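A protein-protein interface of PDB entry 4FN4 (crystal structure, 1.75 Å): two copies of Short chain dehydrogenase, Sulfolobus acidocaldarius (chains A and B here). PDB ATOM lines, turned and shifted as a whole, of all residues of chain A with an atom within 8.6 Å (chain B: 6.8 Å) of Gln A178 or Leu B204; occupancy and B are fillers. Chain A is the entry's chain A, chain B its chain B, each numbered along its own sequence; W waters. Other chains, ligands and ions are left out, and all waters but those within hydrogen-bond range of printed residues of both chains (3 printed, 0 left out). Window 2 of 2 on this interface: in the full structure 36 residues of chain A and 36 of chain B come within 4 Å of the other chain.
Water W1 lies within hydrogen-bond range of the side-chain hydroxyl of Thr B208 (2.6 Å), the backbone carbonyl oxygen of Leu B204 (2.9 Å) and the backbone carbonyl oxygen of His A174 (3.3 Å). Water W2 bridges the side-chain hydroxyl of Tyr A175 (2.6 Å) and the side-chain carboxylate of Glu B103 (2.9 Å). Water W3 lies within hydrogen-bond range of NE2 of His A174 (2.7 Å) and O of Gly B205 (2.7 Å).
No position is printed for both chains.
Of the printed residues of chain B, Gln A178 touches Leu B204 (3.7 Å). Leu B204 touches just these residues of chain A: His A174 (3.7 Å), Tyr A175 (3.4 Å) and Gln A178 (3.7 Å). Of the printed residues of chain B, Tyr A175 touches Pro B100 (3.3 Å) and Leu B204 (3.4 Å). Of the printed residues of chain B, Ala A173 touches Thr B208 (3.8 Å). Printed residues of chain A within 4 Å of Pro B100: His A174 and Tyr A175. Of the printed residues of chain B, His A174 touches Pro B100, Leu B204, Gly B205 and Thr B208. Arg B207 touches none of the printed residues of chain A. Lys A133 touches none of the printed residues of chain B.
Among the printed residues, pairs that only touch across the chains: Ala A173 with Thr B208 (3.8 Å), His A174 with Pro B100 (3.5 Å), His A174 with Leu B204 (3.7 Å), His A174 with Gly B205 (3.97 Å), His A174 with Thr B208 (3.8 Å), Tyr A175 with Pro B100 (3.3 Å), Tyr A175 with Leu B204 (3.4 Å) and Gln A178 with Leu B204 (3.7 Å).
The side-chain hydroxyl (OG) of Ser B202 is in hydrogen-bond range of the backbone NH (N) of Gly B205 (3.2 Å). OE1 of Gln A178 sits close to O of His A174. The backbone NH (N) of Leu B204 lies close to the side-chain hydroxyl (OG) of Ser B202 (3.3 Å). O of Tyr A175 is in hydrogen-bond range of N of Ile A180, at 3.3 Å.
Of the 12 printed residues of chain B, 4 touch a printed residue of chain A. Printed residues of chain B that touch a printed residue of chain A: Pro B100, Leu B204, Gly B205 and Thr B208. Hydrophobic or aromatic side chains of chain B within 4 Å of the printed part of chain A: Pro B100 and Leu B204. Among the printed residues, no Asp or Glu carboxylate lies within 4 Å of a Lys or Arg side-chain nitrogen of the other chain.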
ATOM      1  N   ILE A 128      -3.798   2.546   5.149  1.00  0.00           N
ATOM      2  CA  ILE A 128      -3.601   3.824   4.474  1.00  0.00           C
ATOM      3  C   ILE A 128      -3.405   5.026   5.413  1.00  0.00           C
ATOM      4  O   ILE A 128      -2.489   5.818   5.208  1.00  0.00           O
ATOM      5  CB  ILE A 128      -4.745   4.079   3.441  1.00  0.00           C
ATOM      6  CG1 ILE A 128      -4.480   3.216   2.202  1.00  0.00           C
ATOM      7  CG2 ILE A 128      -4.795   5.557   3.024  1.00  0.00           C
ATOM      8  CD1 ILE A 128      -5.618   3.185   1.188  1.00  0.00           C
ATOM      9  N   ILE A 130      -2.181   5.144   8.337  1.00  0.00           N
ATOM     10  CA  ILE A 130      -0.856   5.016   8.948  1.00  0.00           C
ATOM     11  C   ILE A 130       0.224   5.410   7.933  1.00  0.00           C
ATOM     12  O   ILE A 130       1.195   6.091   8.273  1.00  0.00           O
ATOM     13  CB  ILE A 130      -0.635   3.568   9.449  1.00  0.00           C
ATOM     14  CG1 ILE A 130      -1.589   3.293  10.621  1.00  0.00           C
ATOM     15  CG2 ILE A 130       0.827   3.350   9.864  1.00  0.00           C
ATOM     16  CD1 ILE A 130      -1.665   1.816  11.047  1.00  0.00           C
ATOM     17  N   MET A 131       0.044   5.003   6.679  1.00  0.00           N
ATOM     18  CA  MET A 131       1.017   5.351   5.651  1.00  0.00           C
ATOM     19  C   MET A 131       0.951   6.841   5.318  1.00  0.00           C
ATOM     20  O   MET A 131       1.979   7.466   5.028  1.00  0.00           O
ATOM     21  CB  MET A 131       0.785   4.510   4.395  1.00  0.00           C
ATOM     22  CG  MET A 131       0.952   3.023   4.665  1.00  0.00           C
ATOM     23  SD  MET A 131       0.741   2.021   3.186  1.00  0.00           S
ATOM     24  CE  MET A 131       1.557   0.508   3.711  1.00  0.00           C
ATOM     25  N   LEU A 132      -0.252   7.416   5.340  1.00  0.00           N
ATOM     26  CA  LEU A 132      -0.387   8.845   5.072  1.00  0.00           C
ATOM     27  C   LEU A 132       0.317   9.624   6.184  1.00  0.00           C
ATOM     28  O   LEU A 132       0.959  10.647   5.930  1.00  0.00           O
ATOM     29  CB  LEU A 132      -1.858   9.256   5.006  1.00  0.00           C
ATOM     30  CG  LEU A 132      -2.643   8.701   3.809  1.00  0.00           C
ATOM     31  CD1 LEU A 132      -4.121   9.052   3.953  1.00  0.00           C
ATOM     32  CD2 LEU A 132      -2.083   9.287   2.508  1.00  0.00           C
ATOM     33  N   LYS A 133       0.172   9.149   7.419  1.00  0.00           N
ATOM     34  CA  LYS A 133       0.833   9.786   8.561  1.00  0.00           C
ATOM     35  C   LYS A 133       2.350   9.773   8.324  1.00  0.00           C
ATOM     36  O   LYS A 133       3.049  10.776   8.544  1.00  0.00           O
ATOM     37  CB  LYS A 133       0.507   9.013   9.841  1.00  0.00           C
ATOM     38  CG  LYS A 133       1.252   9.508  11.080  1.00  0.00           C
ATOM     39  CD  LYS A 133       0.924   8.633  12.276  1.00  0.00           C
ATOM     40  CE  LYS A 133       1.586   7.265  12.185  1.00  0.00           C
ATOM     41  NZ  LYS A 133       3.072   7.340  12.365  1.00  0.00           N
ATOM     42  N   GLN A 134       2.855   8.629   7.874  1.00  0.00           N
ATOM     43  CA  GLN A 134       4.281   8.468   7.597  1.00  0.00           C
ATOM     44  C   GLN A 134       4.721   9.259   6.375  1.00  0.00           C
ATOM     45  O   GLN A 134       5.896   9.624   6.255  1.00  0.00           O
ATOM     46  CB  GLN A 134       4.604   6.986   7.378  1.00  0.00           C
ATOM     47  CG  GLN A 134       4.450   6.136   8.639  1.00  0.00           C
ATOM     48  CD  GLN A 134       4.340   4.644   8.364  1.00  0.00           C
ATOM     49  OE1 GLN A 134       4.253   3.843   9.298  1.00  0.00           O
ATOM     50  NE2 GLN A 134       4.341   4.263   7.090  1.00  0.00           N
ATOM     51  N   GLY A 135       3.778   9.529   5.480  1.00  0.00           N
ATOM     52  CA  GLY A 135       4.100  10.240   4.254  1.00  0.00           C
ATOM     53  C   GLY A 135       4.724   9.270   3.262  1.00  0.00           C
ATOM     54  O   GLY A 135       5.259   9.669   2.216  1.00  0.00           O
ATOM     55  N   LYS A 136       4.633   7.980   3.576  1.00  0.00           N
ATOM     56  CA  LYS A 136       5.220   6.961   2.705  1.00  0.00           C
ATOM     57  C   LYS A 136       4.696   5.567   3.025  1.00  0.00           C
ATOM     58  O   LYS A 136       4.541   5.211   4.193  1.00  0.00           O
ATOM     59  CB  LYS A 136       6.749   6.965   2.853  1.00  0.00           C
ATOM     60  CG  LYS A 136       7.474   6.032   1.871  1.00  0.00           C
ATOM     61  CD  LYS A 136       8.984   6.059   2.077  1.00  0.00           C
ATOM     62  CE  LYS A 136       9.687   5.101   1.118  1.00  0.00           C
ATOM     63  NZ  LYS A 136      11.166   5.176   1.262  1.00  0.00           N
ATOM     64  N   GLY A 137       4.426   4.788   1.982  1.00  0.00           N
ATOM     65  CA  GLY A 137       3.958   3.422   2.173  1.00  0.00           C
ATOM     66  C   GLY A 137       3.790   2.742   0.832  1.00  0.00           C
ATOM     67  O   GLY A 137       3.603   3.414  -0.182  1.00  0.00           O
ATOM     68  N   SER A 170      -7.167   2.381  -8.067  1.00  0.00           N
ATOM     69  CA  SER A 170      -7.879   3.388  -7.277  1.00  0.00           C
ATOM     70  C   SER A 170      -6.958   4.003  -6.228  1.00  0.00           C
ATOM     71  O   SER A 170      -6.852   5.230  -6.105  1.00  0.00           O
ATOM     72  CB  SER A 170      -9.093   2.745  -6.603  1.00  0.00           C
ATOM     73  OG  SER A 170      -9.813   3.686  -5.817  1.00  0.00           O
ATOM     74  N   ILE A 171      -6.283   3.145  -5.473  1.00  0.00           N
ATOM     75  CA  ILE A 171      -5.375   3.621  -4.440  1.00  0.00           C
ATOM     76  C   ILE A 171      -4.236   4.440  -5.046  1.00  0.00           C
ATOM     77  O   ILE A 171      -3.875   5.499  -4.519  1.00  0.00           O
ATOM     78  CB  ILE A 171      -4.788   2.441  -3.634  1.00  0.00           C
ATOM     79  CG1 ILE A 171      -5.907   1.752  -2.838  1.00  0.00           C
ATOM     80  CG2 ILE A 171      -3.708   2.955  -2.674  1.00  0.00           C
ATOM     81  CD1 ILE A 171      -5.518   0.378  -2.272  1.00  0.00           C
ATOM     82  N   ALA A 172      -3.666   3.950  -6.144  1.00  0.00           N
ATOM     83  CA  ALA A 172      -2.561   4.654  -6.790  1.00  0.00           C
ATOM     84  C   ALA A 172      -2.995   6.040  -7.251  1.00  0.00           C
ATOM     85  O   ALA A 172      -2.247   7.011  -7.143  1.00  0.00           O
ATOM     86  CB  ALA A 172      -2.053   3.846  -7.988  1.00  0.00           C
ATOM     87  N   ALA A 173      -4.209   6.130  -7.777  1.00  0.00           N
ATOM     88  CA  ALA A 173      -4.710   7.412  -8.261  1.00  0.00           C
ATOM     89  C   ALA A 173      -4.981   8.414  -7.134  1.00  0.00           C
ATOM     90  O   ALA A 173      -4.526   9.563  -7.174  1.00  0.00           O
ATOM     91  CB  ALA A 173      -5.987   7.189  -9.087  1.00  0.00           C
ATOM     92  N   HIS A 174      -5.699   7.975  -6.110  1.00  0.00           N
ATOM     93  CA  HIS A 174      -6.060   8.877  -5.023  1.00  0.00           C
ATOM     94  C   HIS A 174      -4.981   9.218  -4.015  1.00  0.00           C
ATOM     95  O   HIS A 174      -4.984  10.318  -3.447  1.00  0.00           O
ATOM     96  CB  HIS A 174      -7.260   8.308  -4.268  1.00  0.00           C
ATOM     97  CG  HIS A 174      -8.526   8.304  -5.063  1.00  0.00           C
ATOM     98  ND1 HIS A 174      -9.489   7.327  -4.923  1.00  0.00           N
ATOM     99  CD2 HIS A 174      -8.993   9.160  -6.002  1.00  0.00           C
ATOM    100  CE1 HIS A 174     -10.492   7.581  -5.744  1.00  0.00           C
ATOM    101  NE2 HIS A 174     -10.216   8.688  -6.411  1.00  0.00           N
ATOM    102  N   TYR A 175      -4.060   8.294  -3.779  1.00  0.00           N
ATOM    103  CA  TYR A 175      -3.040   8.526  -2.760  1.00  0.00           C
ATOM    104  C   TYR A 175      -1.600   8.640  -3.253  1.00  0.00           C
ATOM    105  O   TYR A 175      -0.676   8.806  -2.450  1.00  0.00           O
ATOM    106  CB  TYR A 175      -3.142   7.425  -1.690  1.00  0.00           C
ATOM    107  CG  TYR A 175      -4.506   7.356  -1.013  1.00  0.00           C
ATOM    108  CD1 TYR A 175      -5.448   6.396  -1.381  1.00  0.00           C
ATOM    109  CD2 TYR A 175      -4.855   8.262  -0.014  1.00  0.00           C
ATOM    110  CE1 TYR A 175      -6.704   6.341  -0.770  1.00  0.00           C
ATOM    111  CE2 TYR A 175      -6.111   8.218   0.603  1.00  0.00           C
ATOM    112  CZ  TYR A 175      -7.025   7.256   0.220  1.00  0.00           C
ATOM    113  OH  TYR A 175      -8.255   7.201   0.825  1.00  0.00           O
ATOM    114  N   GLY A 176      -1.419   8.586  -4.570  1.00  0.00           N
ATOM    115  CA  GLY A 176      -0.083   8.665  -5.131  1.00  0.00           C
ATOM    116  C   GLY A 176       0.671   9.947  -4.817  1.00  0.00           C
ATOM    117  O   GLY A 176       1.899   9.927  -4.715  1.00  0.00           O
ATOM    118  N   ASP A 177      -0.046  11.056  -4.664  1.00  0.00           N
ATOM    119  CA  ASP A 177       0.602  12.336  -4.369  1.00  0.00           C
ATOM    120  C   ASP A 177       0.927  12.505  -2.898  1.00  0.00           C
ATOM    121  O   ASP A 177       1.598  13.464  -2.513  1.00  0.00           O
ATOM    122  CB  ASP A 177      -0.280  13.511  -4.793  1.00  0.00           C
ATOM    123  CG  ASP A 177      -0.389  13.647  -6.292  1.00  0.00           C
ATOM    124  OD1 ASP A 177       0.643  13.504  -6.986  1.00  0.00           O
ATOM    125  OD2 ASP A 177      -1.509  13.912  -6.776  1.00  0.00           O
ATOM    126  N   GLN A 178       0.449  11.576  -2.079  1.00  0.00           N
ATOM    127  CA  GLN A 178       0.670  11.641  -0.647  1.00  0.00           C
ATOM    128  C   GLN A 178       1.705  10.643  -0.134  1.00  0.00           C
ATOM    129  O   GLN A 178       1.796  10.385   1.066  1.00  0.00           O
ATOM    130  CB  GLN A 178      -0.671  11.465   0.066  1.00  0.00           C
ATOM    131  CG  GLN A 178      -1.613  12.640  -0.167  1.00  0.00           C
ATOM    132  CD  GLN A 178      -3.063  12.314   0.140  1.00  0.00           C
ATOM    133  OE1 GLN A 178      -3.770  11.722  -0.682  1.00  0.00           O
ATOM    134  NE2 GLN A 178      -3.514  12.691   1.333  1.00  0.00           N
ATOM    135  N   GLY A 179       2.478  10.078  -1.056  1.00  0.00           N
ATOM    136  CA  GLY A 179       3.526   9.152  -0.674  1.00  0.00           C
ATOM    137  C   GLY A 179       3.192   7.677  -0.708  1.00  0.00           C
ATOM    138  O   GLY A 179       4.015   6.849  -0.325  1.00  0.00           O
ATOM    139  N   ILE A 180       1.997   7.332  -1.162  1.00  0.00           N
ATOM    140  CA  ILE A 180       1.625   5.931  -1.216  1.00  0.00           C
ATOM    141  C   ILE A 180       1.752   5.381  -2.636  1.00  0.00           C
ATOM    142  O   ILE A 180       1.435   6.066  -3.613  1.00  0.00           O
ATOM    143  CB  ILE A 180       0.163   5.719  -0.711  1.00  0.00           C
ATOM    144  CG1 ILE A 180       0.053   6.159   0.755  1.00  0.00           C
ATOM    145  CG2 ILE A 180      -0.252   4.258  -0.872  1.00  0.00           C
ATOM    146  CD1 ILE A 180      -1.278   5.820   1.418  1.00  0.00           C
ATOM    147  N   ARG A 181       2.265   4.162  -2.750  1.00  0.00           N
ATOM    148  CA  ARG A 181       2.346   3.508  -4.047  1.00  0.00           C
ATOM    149  C   ARG A 181       1.560   2.213  -3.896  1.00  0.00           C
ATOM    150  O   ARG A 181       1.654   1.547  -2.876  1.00  0.00           O
ATOM    151  CB  ARG A 181       3.793   3.176  -4.437  1.00  0.00           C
ATOM    152  CG  ARG A 181       4.622   4.406  -4.750  1.00  0.00           C
ATOM    153  CD  ARG A 181       5.920   4.040  -5.443  1.00  0.00           C
ATOM    154  NE  ARG A 181       6.853   3.263  -4.627  1.00  0.00           N
ATOM    155  CZ  ARG A 181       7.066   1.954  -4.758  1.00  0.00           C
ATOM    156  NH1 ARG A 181       6.405   1.243  -5.663  1.00  0.00           N
ATOM    157  NH2 ARG A 181       7.997   1.368  -4.017  1.00  0.00           N
ATOM    158  N   ASN A 241       3.924   3.085  -9.913  1.00  0.00           N
ATOM    159  CA  ASN A 241       2.741   3.269  -9.096  1.00  0.00           C
ATOM    160  C   ASN A 241       1.498   3.033  -9.935  1.00  0.00           C
ATOM    161  O   ASN A 241       1.301   3.690 -10.951  1.00  0.00           O
ATOM    162  CB  ASN A 241       2.709   4.689  -8.511  1.00  0.00           C
ATOM    163  CG  ASN A 241       1.473   4.934  -7.661  1.00  0.00           C
ATOM    164  OD1 ASN A 241       1.027   4.047  -6.937  1.00  0.00           O
ATOM    165  ND2 ASN A 241       0.920   6.144  -7.738  1.00  0.00           N
ATOM    166  N   VAL B  98     -17.516   9.250  -5.043  1.00  0.00           N
ATOM    167  CA  VAL B  98     -16.118   9.431  -5.425  1.00  0.00           C
ATOM    168  C   VAL B  98     -15.284   9.184  -4.168  1.00  0.00           C
ATOM    169  O   VAL B  98     -14.252   9.817  -3.949  1.00  0.00           O
ATOM    170  CB  VAL B  98     -15.861  10.866  -5.952  1.00  0.00           C
ATOM    171  CG1 VAL B  98     -14.563  10.898  -6.757  1.00  0.00           C
ATOM    172  CG2 VAL B  98     -17.025  11.318  -6.831  1.00  0.00           C
ATOM    173  N   PRO B 100     -12.664   7.611  -1.773  1.00  0.00           N
ATOM    174  CA  PRO B 100     -11.394   6.871  -1.819  1.00  0.00           C
ATOM    175  C   PRO B 100     -11.378   5.824  -0.709  1.00  0.00           C
ATOM    176  O   PRO B 100     -12.068   5.973   0.298  1.00  0.00           O
ATOM    177  CB  PRO B 100     -10.345   7.966  -1.634  1.00  0.00           C
ATOM    178  CG  PRO B 100     -11.054   8.953  -0.742  1.00  0.00           C
ATOM    179  CD  PRO B 100     -12.446   9.007  -1.340  1.00  0.00           C
ATOM    180  N   GLU B 103     -11.820   6.227   3.156  1.00  0.00           N
ATOM    181  CA  GLU B 103     -13.069   6.883   3.539  1.00  0.00           C
ATOM    182  C   GLU B 103     -14.316   6.037   3.333  1.00  0.00           C
ATOM    183  O   GLU B 103     -15.420   6.467   3.650  1.00  0.00           O
ATOM    184  CB  GLU B 103     -13.211   8.182   2.740  1.00  0.00           C
ATOM    185  CG  GLU B 103     -12.234   9.258   3.159  1.00  0.00           C
ATOM    186  CD  GLU B 103     -12.166  10.404   2.170  1.00  0.00           C
ATOM    187  OE1 GLU B 103     -13.202  10.746   1.557  1.00  0.00           O
ATOM    188  OE2 GLU B 103     -11.069  10.972   2.017  1.00  0.00           O
ATOM    189  N   PRO B 201     -19.510  14.841  -2.210  1.00  0.00           N
ATOM    190  CA  PRO B 201     -18.536  13.812  -2.562  1.00  0.00           C
ATOM    191  C   PRO B 201     -17.207  14.086  -1.863  1.00  0.00           C
ATOM    192  O   PRO B 201     -16.914  15.227  -1.498  1.00  0.00           O
ATOM    193  CB  PRO B 201     -18.447  13.943  -4.080  1.00  0.00           C
ATOM    194  CG  PRO B 201     -18.687  15.402  -4.300  1.00  0.00           C
ATOM    195  CD  PRO B 201     -19.862  15.654  -3.389  1.00  0.00           C
ATOM    196  N   SER B 202     -16.416  13.037  -1.669  1.00  0.00           N
ATOM    197  CA  SER B 202     -15.114  13.154  -1.018  1.00  0.00           C
ATOM    198  C   SER B 202     -14.258  14.275  -1.616  1.00  0.00           C
ATOM    199  O   SER B 202     -14.110  14.379  -2.837  1.00  0.00           O
ATOM    200  CB  SER B 202     -14.356  11.824  -1.140  1.00  0.00           C
ATOM    201  OG  SER B 202     -13.004  11.963  -0.737  1.00  0.00           O
ATOM    202  N   GLU B 203     -13.695  15.120  -0.758  1.00  0.00           N
ATOM    203  CA  GLU B 203     -12.836  16.190  -1.250  1.00  0.00           C
ATOM    204  C   GLU B 203     -11.610  15.604  -1.953  1.00  0.00           C
ATOM    205  O   GLU B 203     -11.205  16.082  -3.017  1.00  0.00           O
ATOM    206  CB  GLU B 203     -12.405  17.099  -0.099  1.00  0.00           C
ATOM    207  CG  GLU B 203     -13.474  18.105   0.296  1.00  0.00           C
ATOM    208  CD  GLU B 203     -13.108  18.885   1.550  1.00  0.00           C
ATOM    209  OE1 GLU B 203     -11.918  19.247   1.705  1.00  0.00           O
ATOM    210  OE2 GLU B 203     -14.014  19.140   2.375  1.00  0.00           O
ATOM    211  N   LEU B 204     -11.032  14.559  -1.374  1.00  0.00           N
ATOM    212  CA  LEU B 204      -9.850  13.936  -1.973  1.00  0.00           C
ATOM    213  C   LEU B 204     -10.201  13.275  -3.313  1.00  0.00           C
ATOM    214  O   LEU B 204      -9.488  13.434  -4.310  1.00  0.00           O
ATOM    215  CB  LEU B 204      -9.256  12.894  -1.016  1.00  0.00           C
ATOM    216  CG  LEU B 204      -8.049  12.122  -1.568  1.00  0.00           C
ATOM    217  CD1 LEU B 204      -6.929  13.089  -1.900  1.00  0.00           C
ATOM    218  CD2 LEU B 204      -7.581  11.102  -0.550  1.00  0.00           C
ATOM    219  N   GLY B 205     -11.296  12.523  -3.332  1.00  0.00           N
ATOM    220  CA  GLY B 205     -11.707  11.871  -4.566  1.00  0.00           C
ATOM    221  C   GLY B 205     -11.991  12.889  -5.657  1.00  0.00           C
ATOM    222  O   GLY B 205     -11.669  12.673  -6.832  1.00  0.00           O
ATOM    223  N   MET B 206     -12.603  14.007  -5.275  1.00  0.00           N
ATOM    224  CA  MET B 206     -12.923  15.059  -6.239  1.00  0.00           C
ATOM    225  C   MET B 206     -11.680  15.760  -6.766  1.00  0.00           C
ATOM    226  O   MET B 206     -11.673  16.253  -7.892  1.00  0.00           O
ATOM    227  CB  MET B 206     -13.854  16.095  -5.613  1.00  0.00           C
ATOM    228  CG  MET B 206     -15.282  15.636  -5.493  1.00  0.00           C
ATOM    229  SD  MET B 206     -15.984  15.248  -7.109  1.00  0.00           S
ATOM    230  CE  MET B 206     -16.516  16.877  -7.677  1.00  0.00           C
ATOM    231  N   ARG B 207     -10.628  15.821  -5.962  1.00  0.00           N
ATOM    232  CA  ARG B 207      -9.409  16.475  -6.419  1.00  0.00           C
ATOM    233  C   ARG B 207      -8.895  15.771  -7.672  1.00  0.00           C
ATOM    234  O   ARG B 207      -8.366  16.404  -8.586  1.00  0.00           O
ATOM    235  CB  ARG B 207      -8.330  16.455  -5.326  1.00  0.00           C
ATOM    236  CG  ARG B 207      -8.424  17.622  -4.342  1.00  0.00           C
ATOM    237  CD  ARG B 207      -7.171  17.732  -3.469  1.00  0.00           C
ATOM    238  NE  ARG B 207      -7.225  16.877  -2.284  1.00  0.00           N
ATOM    239  CZ  ARG B 207      -8.040  17.082  -1.251  1.00  0.00           C
ATOM    240  NH1 ARG B 207      -8.874  18.116  -1.256  1.00  0.00           N
ATOM    241  NH2 ARG B 207      -8.017  16.257  -0.210  1.00  0.00           N
ATOM    242  N   THR B 208      -9.059  14.457  -7.720  1.00  0.00           N
ATOM    243  CA  THR B 208      -8.602  13.703  -8.874  1.00  0.00           C
ATOM    244  C   THR B 208      -9.590  13.781 -10.032  1.00  0.00           C
ATOM    245  O   THR B 208      -9.193  13.995 -11.174  1.00  0.00           O
ATOM    246  CB  THR B 208      -8.350  12.221  -8.506  1.00  0.00           C
ATOM    247  OG1 THR B 208      -7.253  12.150  -7.584  1.00  0.00           O
ATOM    248  CG2 THR B 208      -7.990  11.402  -9.750  1.00  0.00           C
ATOM    249  N   LEU B 209     -10.876  13.612  -9.737  1.00  0.00           N
ATOM    250  CA  LEU B 209     -11.887  13.645 -10.790  1.00  0.00           C
ATOM    251  C   LEU B 209     -11.901  14.989 -11.513  1.00  0.00           C
ATOM    252  O   LEU B 209     -11.962  15.047 -12.746  1.00  0.00           O
ATOM    253  CB  LEU B 209     -13.274  13.354 -10.204  1.00  0.00           C
ATOM    254  CG  LEU B 209     -14.449  13.355 -11.190  1.00  0.00           C
ATOM    255  CD1 LEU B 209     -14.200  12.324 -12.283  1.00  0.00           C
ATOM    256  CD2 LEU B 209     -15.755  13.056 -10.440  1.00  0.00           C
HETATM  257  O   HOH W   1      -6.831  12.546  -5.053  1.00  0.00           O
HETATM  258  O   HOH W   2      -8.743   9.318   2.281  1.00  0.00           O
HETATM  259  O   HOH W   3     -11.445  10.312  -8.193  1.00  0.00           O
